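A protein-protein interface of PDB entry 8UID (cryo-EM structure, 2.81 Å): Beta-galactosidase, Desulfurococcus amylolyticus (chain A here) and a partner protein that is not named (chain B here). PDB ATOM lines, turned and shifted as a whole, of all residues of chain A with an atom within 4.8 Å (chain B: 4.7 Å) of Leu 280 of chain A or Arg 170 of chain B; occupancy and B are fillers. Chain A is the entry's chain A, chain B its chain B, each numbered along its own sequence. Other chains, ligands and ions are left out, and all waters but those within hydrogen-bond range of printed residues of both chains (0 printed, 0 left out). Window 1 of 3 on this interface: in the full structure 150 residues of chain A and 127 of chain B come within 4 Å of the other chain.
OG of Ser 282 of chain A sits at hydrogen-bond distance from N of Arg 170 of chain B.
NH2 of Arg 170 of chain B lies within hydrogen-bond range of O of Thr 676 of chain A (2.9 Å).
O of Glu 92 of chain A sits at hydrogen-bond distance from N of Ala 277 of chain A, at 3.0 Å.
The side-chain carboxylate of Glu 92 of chain A is in hydrogen-bond range of the side-chain hydroxyl of Tyr 284 of chain A (2.5 Å).
O of Tyr 279 of chain A is in hydrogen-bond range of N of Ser 229 of chain A (2.8 Å).
The side-chain amide nitrogen (ND2) of Asn 271 of chain A lies close to the side-chain hydroxyl (OG1) of Thr 276 of chain A (3.4 Å).
The backbone NH (N) of Asn 271 of chain A sits at hydrogen-bond distance from the backbone carbonyl oxygen (O) of Ser 282 of chain A (2.9 Å).
The side-chain carboxylate (OE2) of Glu 674 of chain A lies within hydrogen-bond range of the side-chain hydroxyl (OH) of Tyr 274 of chain A (2.6 Å).
Among the printed residues, merely in contact across the chains: Lys 278 of chain A with Asn 35 of chain B, Tyr 274 of chain A with Leu 160 of chain B, Tyr 274 of chain A with Arg 170 of chain B, Phe 226 of chain A with Asn 35 of chain B, Thr 276 of chain A with Arg 170 of chain B, Ser 282 of chain A with Gly 169 of chain B, Gly 273 of chain A with Phe 167 of chain B, Gly 273 of chain A with Arg 170 of chain B, Leu 280 of chain A with Arg 170 of chain B, Tyr 279 of chain A with Asn 35 of chain B, Leu 280 of chain A with Asn 35 of chain B, Glu 92 of chain A with Asn 35 of chain B, Ser 228 of chain A with Asn 35 of chain B and Ala 277 of chain A with Asn 35 of chain B.
Leu 280 of chain A touches just these residues of chain B: Asn 35 (3.9 Å) and Arg 170 (3.7 Å).
Arg 170 of chain B touches just these residues of chain A: Gly 273, Tyr 274, Thr 276, Leu 280, Ser 282 and Thr 676.
Of the printed residues of chain B, Ser 282 of chain A touches Gly 169 (3.3 Å) and Arg 170 (3.1 Å).
Printed residues of chain B within 4 Å of Tyr 274 of chain A: Leu 160 and Arg 170.
Of the printed residues of chain A, Asn 35 of chain B touches Glu 92, Phe 226, Ser 228, Ala 277, Lys 278, Tyr 279 and Leu 280.
Of the printed residues of chain B, Thr 276 of chain A touches Arg 170 (3.3 Å).
Tyr 284 of chain A touches none of the printed residues of chain B.
Lys 227 of chain A touches none of the printed residues of chain B.
Of the 18 printed residues of chain A, 12 touch a printed residue of chain B.
Hydrophobic or aromatic side chains of chain A within 4 Å of the printed part of chain B: Phe 226, Tyr 274, Ala 277, Tyr 279 and Leu 280.
Printed residues of chain B that touch a printed residue of chain A: Asn 35, Leu 160, Phe 167, Gly 169 and Arg 170.
Hydrophobic or aromatic side chains of chain B that line the printed part of chain A: Leu 160 and Phe 167.
Among the printed residues, 16 pairs touch across the chains.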
ATOM      1  N   GLU A  92      15.702  14.725  -8.401  1.00  0.00           N
ATOM      2  CA  GLU A  92      15.373  13.531  -7.639  1.00  0.00           C
ATOM      3  C   GLU A  92      15.165  12.308  -8.535  1.00  0.00           C
ATOM      4  O   GLU A  92      14.388  11.400  -8.256  1.00  0.00           O
ATOM      5  CB  GLU A  92      14.239  13.809  -6.664  1.00  0.00           C
ATOM      6  CG  GLU A  92      14.531  14.939  -5.671  1.00  0.00           C
ATOM      7  CD  GLU A  92      14.493  16.343  -6.297  1.00  0.00           C
ATOM      8  OE1 GLU A  92      15.467  17.111  -6.127  1.00  0.00           O
ATOM      9  OE2 GLU A  92      13.504  16.669  -6.992  1.00  0.00           O
ATOM     10  N   PHE A 226       9.462  17.407  -2.659  1.00  0.00           N
ATOM     11  CA  PHE A 226       9.332  15.960  -2.848  1.00  0.00           C
ATOM     12  C   PHE A 226       9.157  15.193  -1.530  1.00  0.00           C
ATOM     13  O   PHE A 226       9.339  15.740  -0.446  1.00  0.00           O
ATOM     14  CB  PHE A 226      10.519  15.448  -3.664  1.00  0.00           C
ATOM     15  CG  PHE A 226      11.861  15.689  -3.025  1.00  0.00           C
ATOM     16  CD1 PHE A 226      12.382  14.760  -2.115  1.00  0.00           C
ATOM     17  CD2 PHE A 226      12.588  16.846  -3.344  1.00  0.00           C
ATOM     18  CE1 PHE A 226      13.622  14.997  -1.512  1.00  0.00           C
ATOM     19  CE2 PHE A 226      13.845  17.061  -2.770  1.00  0.00           C
ATOM     20  CZ  PHE A 226      14.359  16.141  -1.849  1.00  0.00           C
ATOM     21  N   LYS A 227       8.809  13.904  -1.618  1.00  0.00           N
ATOM     22  CA  LYS A 227       8.697  12.977  -0.484  1.00  0.00           C
ATOM     23  C   LYS A 227       9.625  11.783  -0.671  1.00  0.00           C
ATOM     24  O   LYS A 227       9.856  11.326  -1.785  1.00  0.00           O
ATOM     25  CB  LYS A 227       7.227  12.607  -0.202  1.00  0.00           C
ATOM     26  CG  LYS A 227       6.616  11.608  -1.205  1.00  0.00           C
ATOM     27  CD  LYS A 227       5.085  11.529  -1.116  1.00  0.00           C
ATOM     28  CE  LYS A 227       4.446  12.729  -1.834  1.00  0.00           C
ATOM     29  NZ  LYS A 227       3.015  12.915  -1.469  1.00  0.00           N
ATOM     30  N   SER A 228      10.173  11.277   0.418  1.00  0.00           N
ATOM     31  CA  SER A 228      11.163  10.200   0.437  1.00  0.00           C
ATOM     32  C   SER A 228      10.739   9.081   1.365  1.00  0.00           C
ATOM     33  O   SER A 228      10.009   9.319   2.319  1.00  0.00           O
ATOM     34  CB  SER A 228      12.525  10.724   0.890  1.00  0.00           C
ATOM     35  OG  SER A 228      12.945  11.784   0.053  1.00  0.00           O
ATOM     36  N   SER A 229      11.212   7.865   1.133  1.00  0.00           N
ATOM     37  CA  SER A 229      11.294   6.877   2.202  1.00  0.00           C
ATOM     38  C   SER A 229      12.454   7.209   3.149  1.00  0.00           C
ATOM     39  O   SER A 229      13.228   8.136   2.912  1.00  0.00           O
ATOM     40  CB  SER A 229      11.392   5.472   1.608  1.00  0.00           C
ATOM     41  OG  SER A 229      12.559   5.318   0.841  1.00  0.00           O
ATOM     42  N   ASN A 271       7.493   8.818 -10.610  1.00  0.00           N
ATOM     43  CA  ASN A 271       8.741   8.206 -11.052  1.00  0.00           C
ATOM     44  C   ASN A 271       8.479   6.825 -11.691  1.00  0.00           C
ATOM     45  O   ASN A 271       7.908   5.977 -11.008  1.00  0.00           O
ATOM     46  CB  ASN A 271       9.680   8.081  -9.852  1.00  0.00           C
ATOM     47  CG  ASN A 271      10.402   9.366  -9.516  1.00  0.00           C
ATOM     48  OD1 ASN A 271      10.072  10.089  -8.600  1.00  0.00           O
ATOM     49  ND2 ASN A 271      11.443   9.687 -10.240  1.00  0.00           N
ATOM     50  N   GLY A 273       9.069   3.488 -11.933  1.00  0.00           N
ATOM     51  CA  GLY A 273       9.727   2.397 -11.237  1.00  0.00           C
ATOM     52  C   GLY A 273      11.043   2.820 -10.611  1.00  0.00           C
ATOM     53  O   GLY A 273      11.073   3.628  -9.687  1.00  0.00           O
ATOM     54  N   TYR A 274      12.140   2.239 -11.084  1.00  0.00           N
ATOM     55  CA  TYR A 274      13.472   2.465 -10.544  1.00  0.00           C
ATOM     56  C   TYR A 274      14.242   3.618 -11.188  1.00  0.00           C
ATOM     57  O   TYR A 274      15.359   3.905 -10.779  1.00  0.00           O
ATOM     58  CB  TYR A 274      14.228   1.144 -10.516  1.00  0.00           C
ATOM     59  CG  TYR A 274      13.693   0.225  -9.450  1.00  0.00           C
ATOM     60  CD1 TYR A 274      14.180   0.356  -8.140  1.00  0.00           C
ATOM     61  CD2 TYR A 274      12.693  -0.714  -9.746  1.00  0.00           C
ATOM     62  CE1 TYR A 274      13.651  -0.441  -7.115  1.00  0.00           C
ATOM     63  CE2 TYR A 274      12.153  -1.506  -8.721  1.00  0.00           C
ATOM     64  CZ  TYR A 274      12.633  -1.370  -7.408  1.00  0.00           C
ATOM     65  OH  TYR A 274      12.095  -2.122  -6.432  1.00  0.00           O
ATOM     66  N   THR A 276      14.368   6.685 -10.249  1.00  0.00           N
ATOM     67  CA  THR A 276      14.160   7.592  -9.138  1.00  0.00           C
ATOM     68  C   THR A 276      15.442   7.682  -8.343  1.00  0.00           C
ATOM     69  O   THR A 276      16.301   6.817  -8.481  1.00  0.00           O
ATOM     70  CB  THR A 276      12.969   7.125  -8.314  1.00  0.00           C
ATOM     71  OG1 THR A 276      12.605   8.169  -7.470  1.00  0.00           O
ATOM     72  CG2 THR A 276      13.199   5.885  -7.477  1.00  0.00           C
ATOM     73  N   ALA A 277      15.623   8.731  -7.555  1.00  0.00           N
ATOM     74  CA  ALA A 277      16.821   8.829  -6.753  1.00  0.00           C
ATOM     75  C   ALA A 277      16.827   7.761  -5.661  1.00  0.00           C
ATOM     76  O   ALA A 277      15.800   7.195  -5.287  1.00  0.00           O
ATOM     77  CB  ALA A 277      16.927  10.220  -6.157  1.00  0.00           C
ATOM     78  N   LYS A 278      17.980   7.544  -5.050  1.00  0.00           N
ATOM     79  CA  LYS A 278      18.071   6.749  -3.833  1.00  0.00           C
ATOM     80  C   LYS A 278      17.094   7.293  -2.765  1.00  0.00           C
ATOM     81  O   LYS A 278      16.988   8.501  -2.574  1.00  0.00           O
ATOM     82  CB  LYS A 278      19.544   6.704  -3.398  1.00  0.00           C
ATOM     83  CG  LYS A 278      19.851   5.389  -2.690  1.00  0.00           C
ATOM     84  CD  LYS A 278      21.340   5.177  -2.373  1.00  0.00           C
ATOM     85  CE  LYS A 278      22.261   4.787  -3.542  1.00  0.00           C
ATOM     86  NZ  LYS A 278      21.808   3.587  -4.291  1.00  0.00           N
ATOM     87  N   TYR A 279      16.357   6.412  -2.093  1.00  0.00           N
ATOM     88  CA  TYR A 279      15.322   6.723  -1.085  1.00  0.00           C
ATOM     89  C   TYR A 279      14.109   7.537  -1.552  1.00  0.00           C
ATOM     90  O   TYR A 279      13.353   7.995  -0.703  1.00  0.00           O
ATOM     91  CB  TYR A 279      15.911   7.341   0.195  1.00  0.00           C
ATOM     92  CG  TYR A 279      17.320   6.925   0.513  1.00  0.00           C
ATOM     93  CD1 TYR A 279      17.568   5.611   0.932  1.00  0.00           C
ATOM     94  CD2 TYR A 279      18.381   7.811   0.260  1.00  0.00           C
ATOM     95  CE1 TYR A 279      18.892   5.167   1.057  1.00  0.00           C
ATOM     96  CE2 TYR A 279      19.704   7.378   0.403  1.00  0.00           C
ATOM     97  CZ  TYR A 279      19.954   6.051   0.784  1.00  0.00           C
ATOM     98  OH  TYR A 279      21.230   5.601   0.816  1.00  0.00           O
ATOM     99  N   LEU A 280      13.877   7.790  -2.841  1.00  0.00           N
ATOM    100  CA  LEU A 280      12.656   8.507  -3.224  1.00  0.00           C
ATOM    101  C   LEU A 280      11.421   7.601  -3.265  1.00  0.00           C
ATOM    102  O   LEU A 280      11.520   6.402  -3.519  1.00  0.00           O
ATOM    103  CB  LEU A 280      12.817   9.263  -4.540  1.00  0.00           C
ATOM    104  CG  LEU A 280      12.524  10.750  -4.340  1.00  0.00           C
ATOM    105  CD1 LEU A 280      13.775  11.453  -3.830  1.00  0.00           C
ATOM    106  CD2 LEU A 280      11.986  11.363  -5.622  1.00  0.00           C
ATOM    107  N   ALA A 281      10.246   8.195  -3.063  1.00  0.00           N
ATOM    108  CA  ALA A 281       8.976   7.520  -3.283  1.00  0.00           C
ATOM    109  C   ALA A 281       8.671   7.386  -4.789  1.00  0.00           C
ATOM    110  O   ALA A 281       9.204   8.133  -5.604  1.00  0.00           O
ATOM    111  CB  ALA A 281       7.906   8.302  -2.518  1.00  0.00           C
ATOM    112  N   SER A 282       7.804   6.450  -5.191  1.00  0.00           N
ATOM    113  CA  SER A 282       7.342   6.381  -6.590  1.00  0.00           C
ATOM    114  C   SER A 282       6.419   7.541  -6.967  1.00  0.00           C
ATOM    115  O   SER A 282       6.402   7.978  -8.114  1.00  0.00           O
ATOM    116  CB  SER A 282       6.669   5.046  -6.882  1.00  0.00           C
ATOM    117  OG  SER A 282       7.648   4.021  -6.831  1.00  0.00           O
ATOM    118  N   TYR A 284       6.022  11.289  -7.381  1.00  0.00           N
ATOM    119  CA  TYR A 284       6.658  12.604  -7.484  1.00  0.00           C
ATOM    120  C   TYR A 284       5.590  13.691  -7.525  1.00  0.00           C
ATOM    121  O   TYR A 284       5.750  14.699  -8.188  1.00  0.00           O
ATOM    122  CB  TYR A 284       7.671  12.672  -8.629  1.00  0.00           C
ATOM    123  CG  TYR A 284       8.664  13.824  -8.546  1.00  0.00           C
ATOM    124  CD1 TYR A 284       9.670  13.844  -7.561  1.00  0.00           C
ATOM    125  CD2 TYR A 284       8.633  14.845  -9.507  1.00  0.00           C
ATOM    126  CE1 TYR A 284      10.655  14.851  -7.570  1.00  0.00           C
ATOM    127  CE2 TYR A 284       9.633  15.828  -9.537  1.00  0.00           C
ATOM    128  CZ  TYR A 284      10.655  15.831  -8.582  1.00  0.00           C
ATOM    129  OH  TYR A 284      11.634  16.764  -8.690  1.00  0.00           O
ATOM    130  N   GLU A 674      17.635  -4.879  -3.165  1.00  0.00           N
ATOM    131  CA  GLU A 674      16.913  -3.905  -3.970  1.00  0.00           C
ATOM    132  C   GLU A 674      17.662  -2.581  -3.972  1.00  0.00           C
ATOM    133  O   GLU A 674      17.791  -1.942  -2.942  1.00  0.00           O
ATOM    134  CB  GLU A 674      15.495  -3.741  -3.425  1.00  0.00           C
ATOM    135  CG  GLU A 674      14.666  -2.798  -4.296  1.00  0.00           C
ATOM    136  CD  GLU A 674      13.392  -2.325  -3.598  1.00  0.00           C
ATOM    137  OE1 GLU A 674      12.969  -2.912  -2.580  1.00  0.00           O
ATOM    138  OE2 GLU A 674      12.816  -1.321  -4.070  1.00  0.00           O
ATOM    139  N   THR A 676      17.285   1.126  -4.932  1.00  0.00           N
ATOM    140  CA  THR A 676      16.161   2.064  -5.073  1.00  0.00           C
ATOM    141  C   THR A 676      16.374   3.102  -6.170  1.00  0.00           C
ATOM    142  O   THR A 676      15.433   3.766  -6.583  1.00  0.00           O
ATOM    143  CB  THR A 676      15.917   2.750  -3.719  1.00  0.00           C
ATOM    144  OG1 THR A 676      15.621   1.766  -2.764  1.00  0.00           O
ATOM    145  CG2 THR A 676      14.762   3.741  -3.636  1.00  0.00           C
ATOM    146  N   ASN B  35      19.054  11.515  -0.533  1.00  0.00           N
ATOM    147  CA  ASN B  35      18.795  11.238  -1.952  1.00  0.00           C
ATOM    148  C   ASN B  35      19.764  11.975  -2.868  1.00  0.00           C
ATOM    149  O   ASN B  35      20.005  11.518  -3.981  1.00  0.00           O
ATOM    150  CB  ASN B  35      17.346  11.575  -2.347  1.00  0.00           C
ATOM    151  CG  ASN B  35      16.970  13.020  -2.130  1.00  0.00           C
ATOM    152  OD1 ASN B  35      17.190  13.871  -2.969  1.00  0.00           O
ATOM    153  ND2 ASN B  35      16.424  13.341  -0.990  1.00  0.00           N
ATOM    154  N   ILE B 159       7.129  -3.942  -1.115  1.00  0.00           N
ATOM    155  CA  ILE B 159       6.102  -4.404  -2.045  1.00  0.00           C
ATOM    156  C   ILE B 159       6.202  -3.596  -3.331  1.00  0.00           C
ATOM    157  O   ILE B 159       6.196  -2.369  -3.298  1.00  0.00           O
ATOM    158  CB  ILE B 159       4.683  -4.486  -1.412  1.00  0.00           C
ATOM    159  CG1 ILE B 159       3.999  -3.143  -1.102  1.00  0.00           C
ATOM    160  CG2 ILE B 159       4.714  -5.283  -0.107  1.00  0.00           C
ATOM    161  CD1 ILE B 159       3.040  -2.745  -2.212  1.00  0.00           C
ATOM    162  N   LEU B 160       6.304  -4.283  -4.462  1.00  0.00           N
ATOM    163  CA  LEU B 160       6.200  -3.687  -5.789  1.00  0.00           C
ATOM    164  C   LEU B 160       4.799  -3.936  -6.319  1.00  0.00           C
ATOM    165  O   LEU B 160       4.320  -5.061  -6.268  1.00  0.00           O
ATOM    166  CB  LEU B 160       7.221  -4.252  -6.784  1.00  0.00           C
ATOM    167  CG  LEU B 160       8.585  -4.717  -6.280  1.00  0.00           C
ATOM    168  CD1 LEU B 160       9.410  -5.169  -7.483  1.00  0.00           C
ATOM    169  CD2 LEU B 160       9.365  -3.636  -5.555  1.00  0.00           C
ATOM    170  N   PHE B 167       3.842  -1.677 -14.292  1.00  0.00           N
ATOM    171  CA  PHE B 167       4.503  -1.394 -13.017  1.00  0.00           C
ATOM    172  C   PHE B 167       4.086  -0.030 -12.469  1.00  0.00           C
ATOM    173  O   PHE B 167       4.362   0.997 -13.088  1.00  0.00           O
ATOM    174  CB  PHE B 167       6.024  -1.441 -13.204  1.00  0.00           C
ATOM    175  CG  PHE B 167       6.788  -1.378 -11.898  1.00  0.00           C
ATOM    176  CD1 PHE B 167       7.066  -0.164 -11.249  1.00  0.00           C
ATOM    177  CD2 PHE B 167       7.181  -2.571 -11.293  1.00  0.00           C
ATOM    178  CE1 PHE B 167       7.681  -0.170  -9.985  1.00  0.00           C
ATOM    179  CE2 PHE B 167       7.796  -2.578 -10.041  1.00  0.00           C
ATOM    180  CZ  PHE B 167       8.053  -1.377  -9.381  1.00  0.00           C
ATOM    181  N   GLY B 169       4.575   1.139  -8.902  1.00  0.00           N
ATOM    182  CA  GLY B 169       5.454   1.728  -7.899  1.00  0.00           C
ATOM    183  C   GLY B 169       5.877   0.783  -6.791  1.00  0.00           C
ATOM    184  O   GLY B 169       5.578  -0.403  -6.822  1.00  0.00           O
ATOM    185  N   ARG B 170       6.569   1.326  -5.792  1.00  0.00           N
ATOM    186  CA  ARG B 170       7.037   0.599  -4.606  1.00  0.00           C
ATOM    187  C   ARG B 170       6.473   1.216  -3.338  1.00  0.00           C
ATOM    188  O   ARG B 170       6.306   2.427  -3.260  1.00  0.00           O
ATOM    189  CB  ARG B 170       8.574   0.534  -4.509  1.00  0.00           C
ATOM    190  CG  ARG B 170       9.268  -0.039  -5.747  1.00  0.00           C
ATOM    191  CD  ARG B 170       9.603   0.997  -6.827  1.00  0.00           C
ATOM    192  NE  ARG B 170      11.002   1.459  -6.772  1.00  0.00           N
ATOM    193  CZ  ARG B 170      11.532   2.480  -6.131  1.00  0.00           C
ATOM    194  NH1 ARG B 170      10.893   3.218  -5.281  1.00  0.00           N
ATOM    195  NH2 ARG B 170      12.764   2.779  -6.376  1.00  0.00           N
ATOM    196  N   ILE B 171       6.232   0.388  -2.335  1.00  0.00           N
ATOM    197  CA  ILE B 171       5.903   0.825  -0.984  1.00  0.00           C
ATOM    198  C   ILE B 171       6.743   0.008   0.001  1.00  0.00           C
ATOM    199  O   ILE B 171       6.966  -1.184  -0.188  1.00  0.00           O
ATOM    200  CB  ILE B 171       4.379   0.778  -0.701  1.00  0.00           C
ATOM    201  CG1 ILE B 171       3.488   1.092  -1.927  1.00  0.00           C
ATOM    202  CG2 ILE B 171       4.067   1.768   0.434  1.00  0.00           C
ATOM    203  CD1 ILE B 171       1.982   1.080  -1.651  1.00  0.00           C
ATOM    204  N   SER B 172       7.222   0.645   1.060  1.00  0.00           N
ATOM    205  CA  SER B 172       8.050   0.042   2.110  1.00  0.00           C
ATOM    206  C   SER B 172       7.576   0.511   3.482  1.00  0.00           C
ATOM    207  O   SER B 172       6.858   1.505   3.569  1.00  0.00           O
ATOM    208  CB  SER B 172       9.521   0.392   1.848  1.00  0.00           C
ATOM    209  OG  SER B 172       9.768   1.785   1.876  1.00  0.00           O
ATOM    210  N   LEU B 180      -0.438   4.486  -3.813  1.00  0.00           N
ATOM    211  CA  LEU B 180       0.106   4.766  -5.139  1.00  0.00           C
ATOM    212  C   LEU B 180      -0.986   5.267  -6.073  1.00  0.00           C
ATOM    213  O   LEU B 180      -2.016   4.625  -6.201  1.00  0.00           O
ATOM    214  CB  LEU B 180       0.733   3.490  -5.715  1.00  0.00           C
ATOM    215  CG  LEU B 180       2.005   3.028  -5.001  1.00  0.00           C
ATOM    216  CD1 LEU B 180       2.379   1.666  -5.557  1.00  0.00           C
ATOM    217  CD2 LEU B 180       3.176   3.977  -5.224  1.00  0.00           C
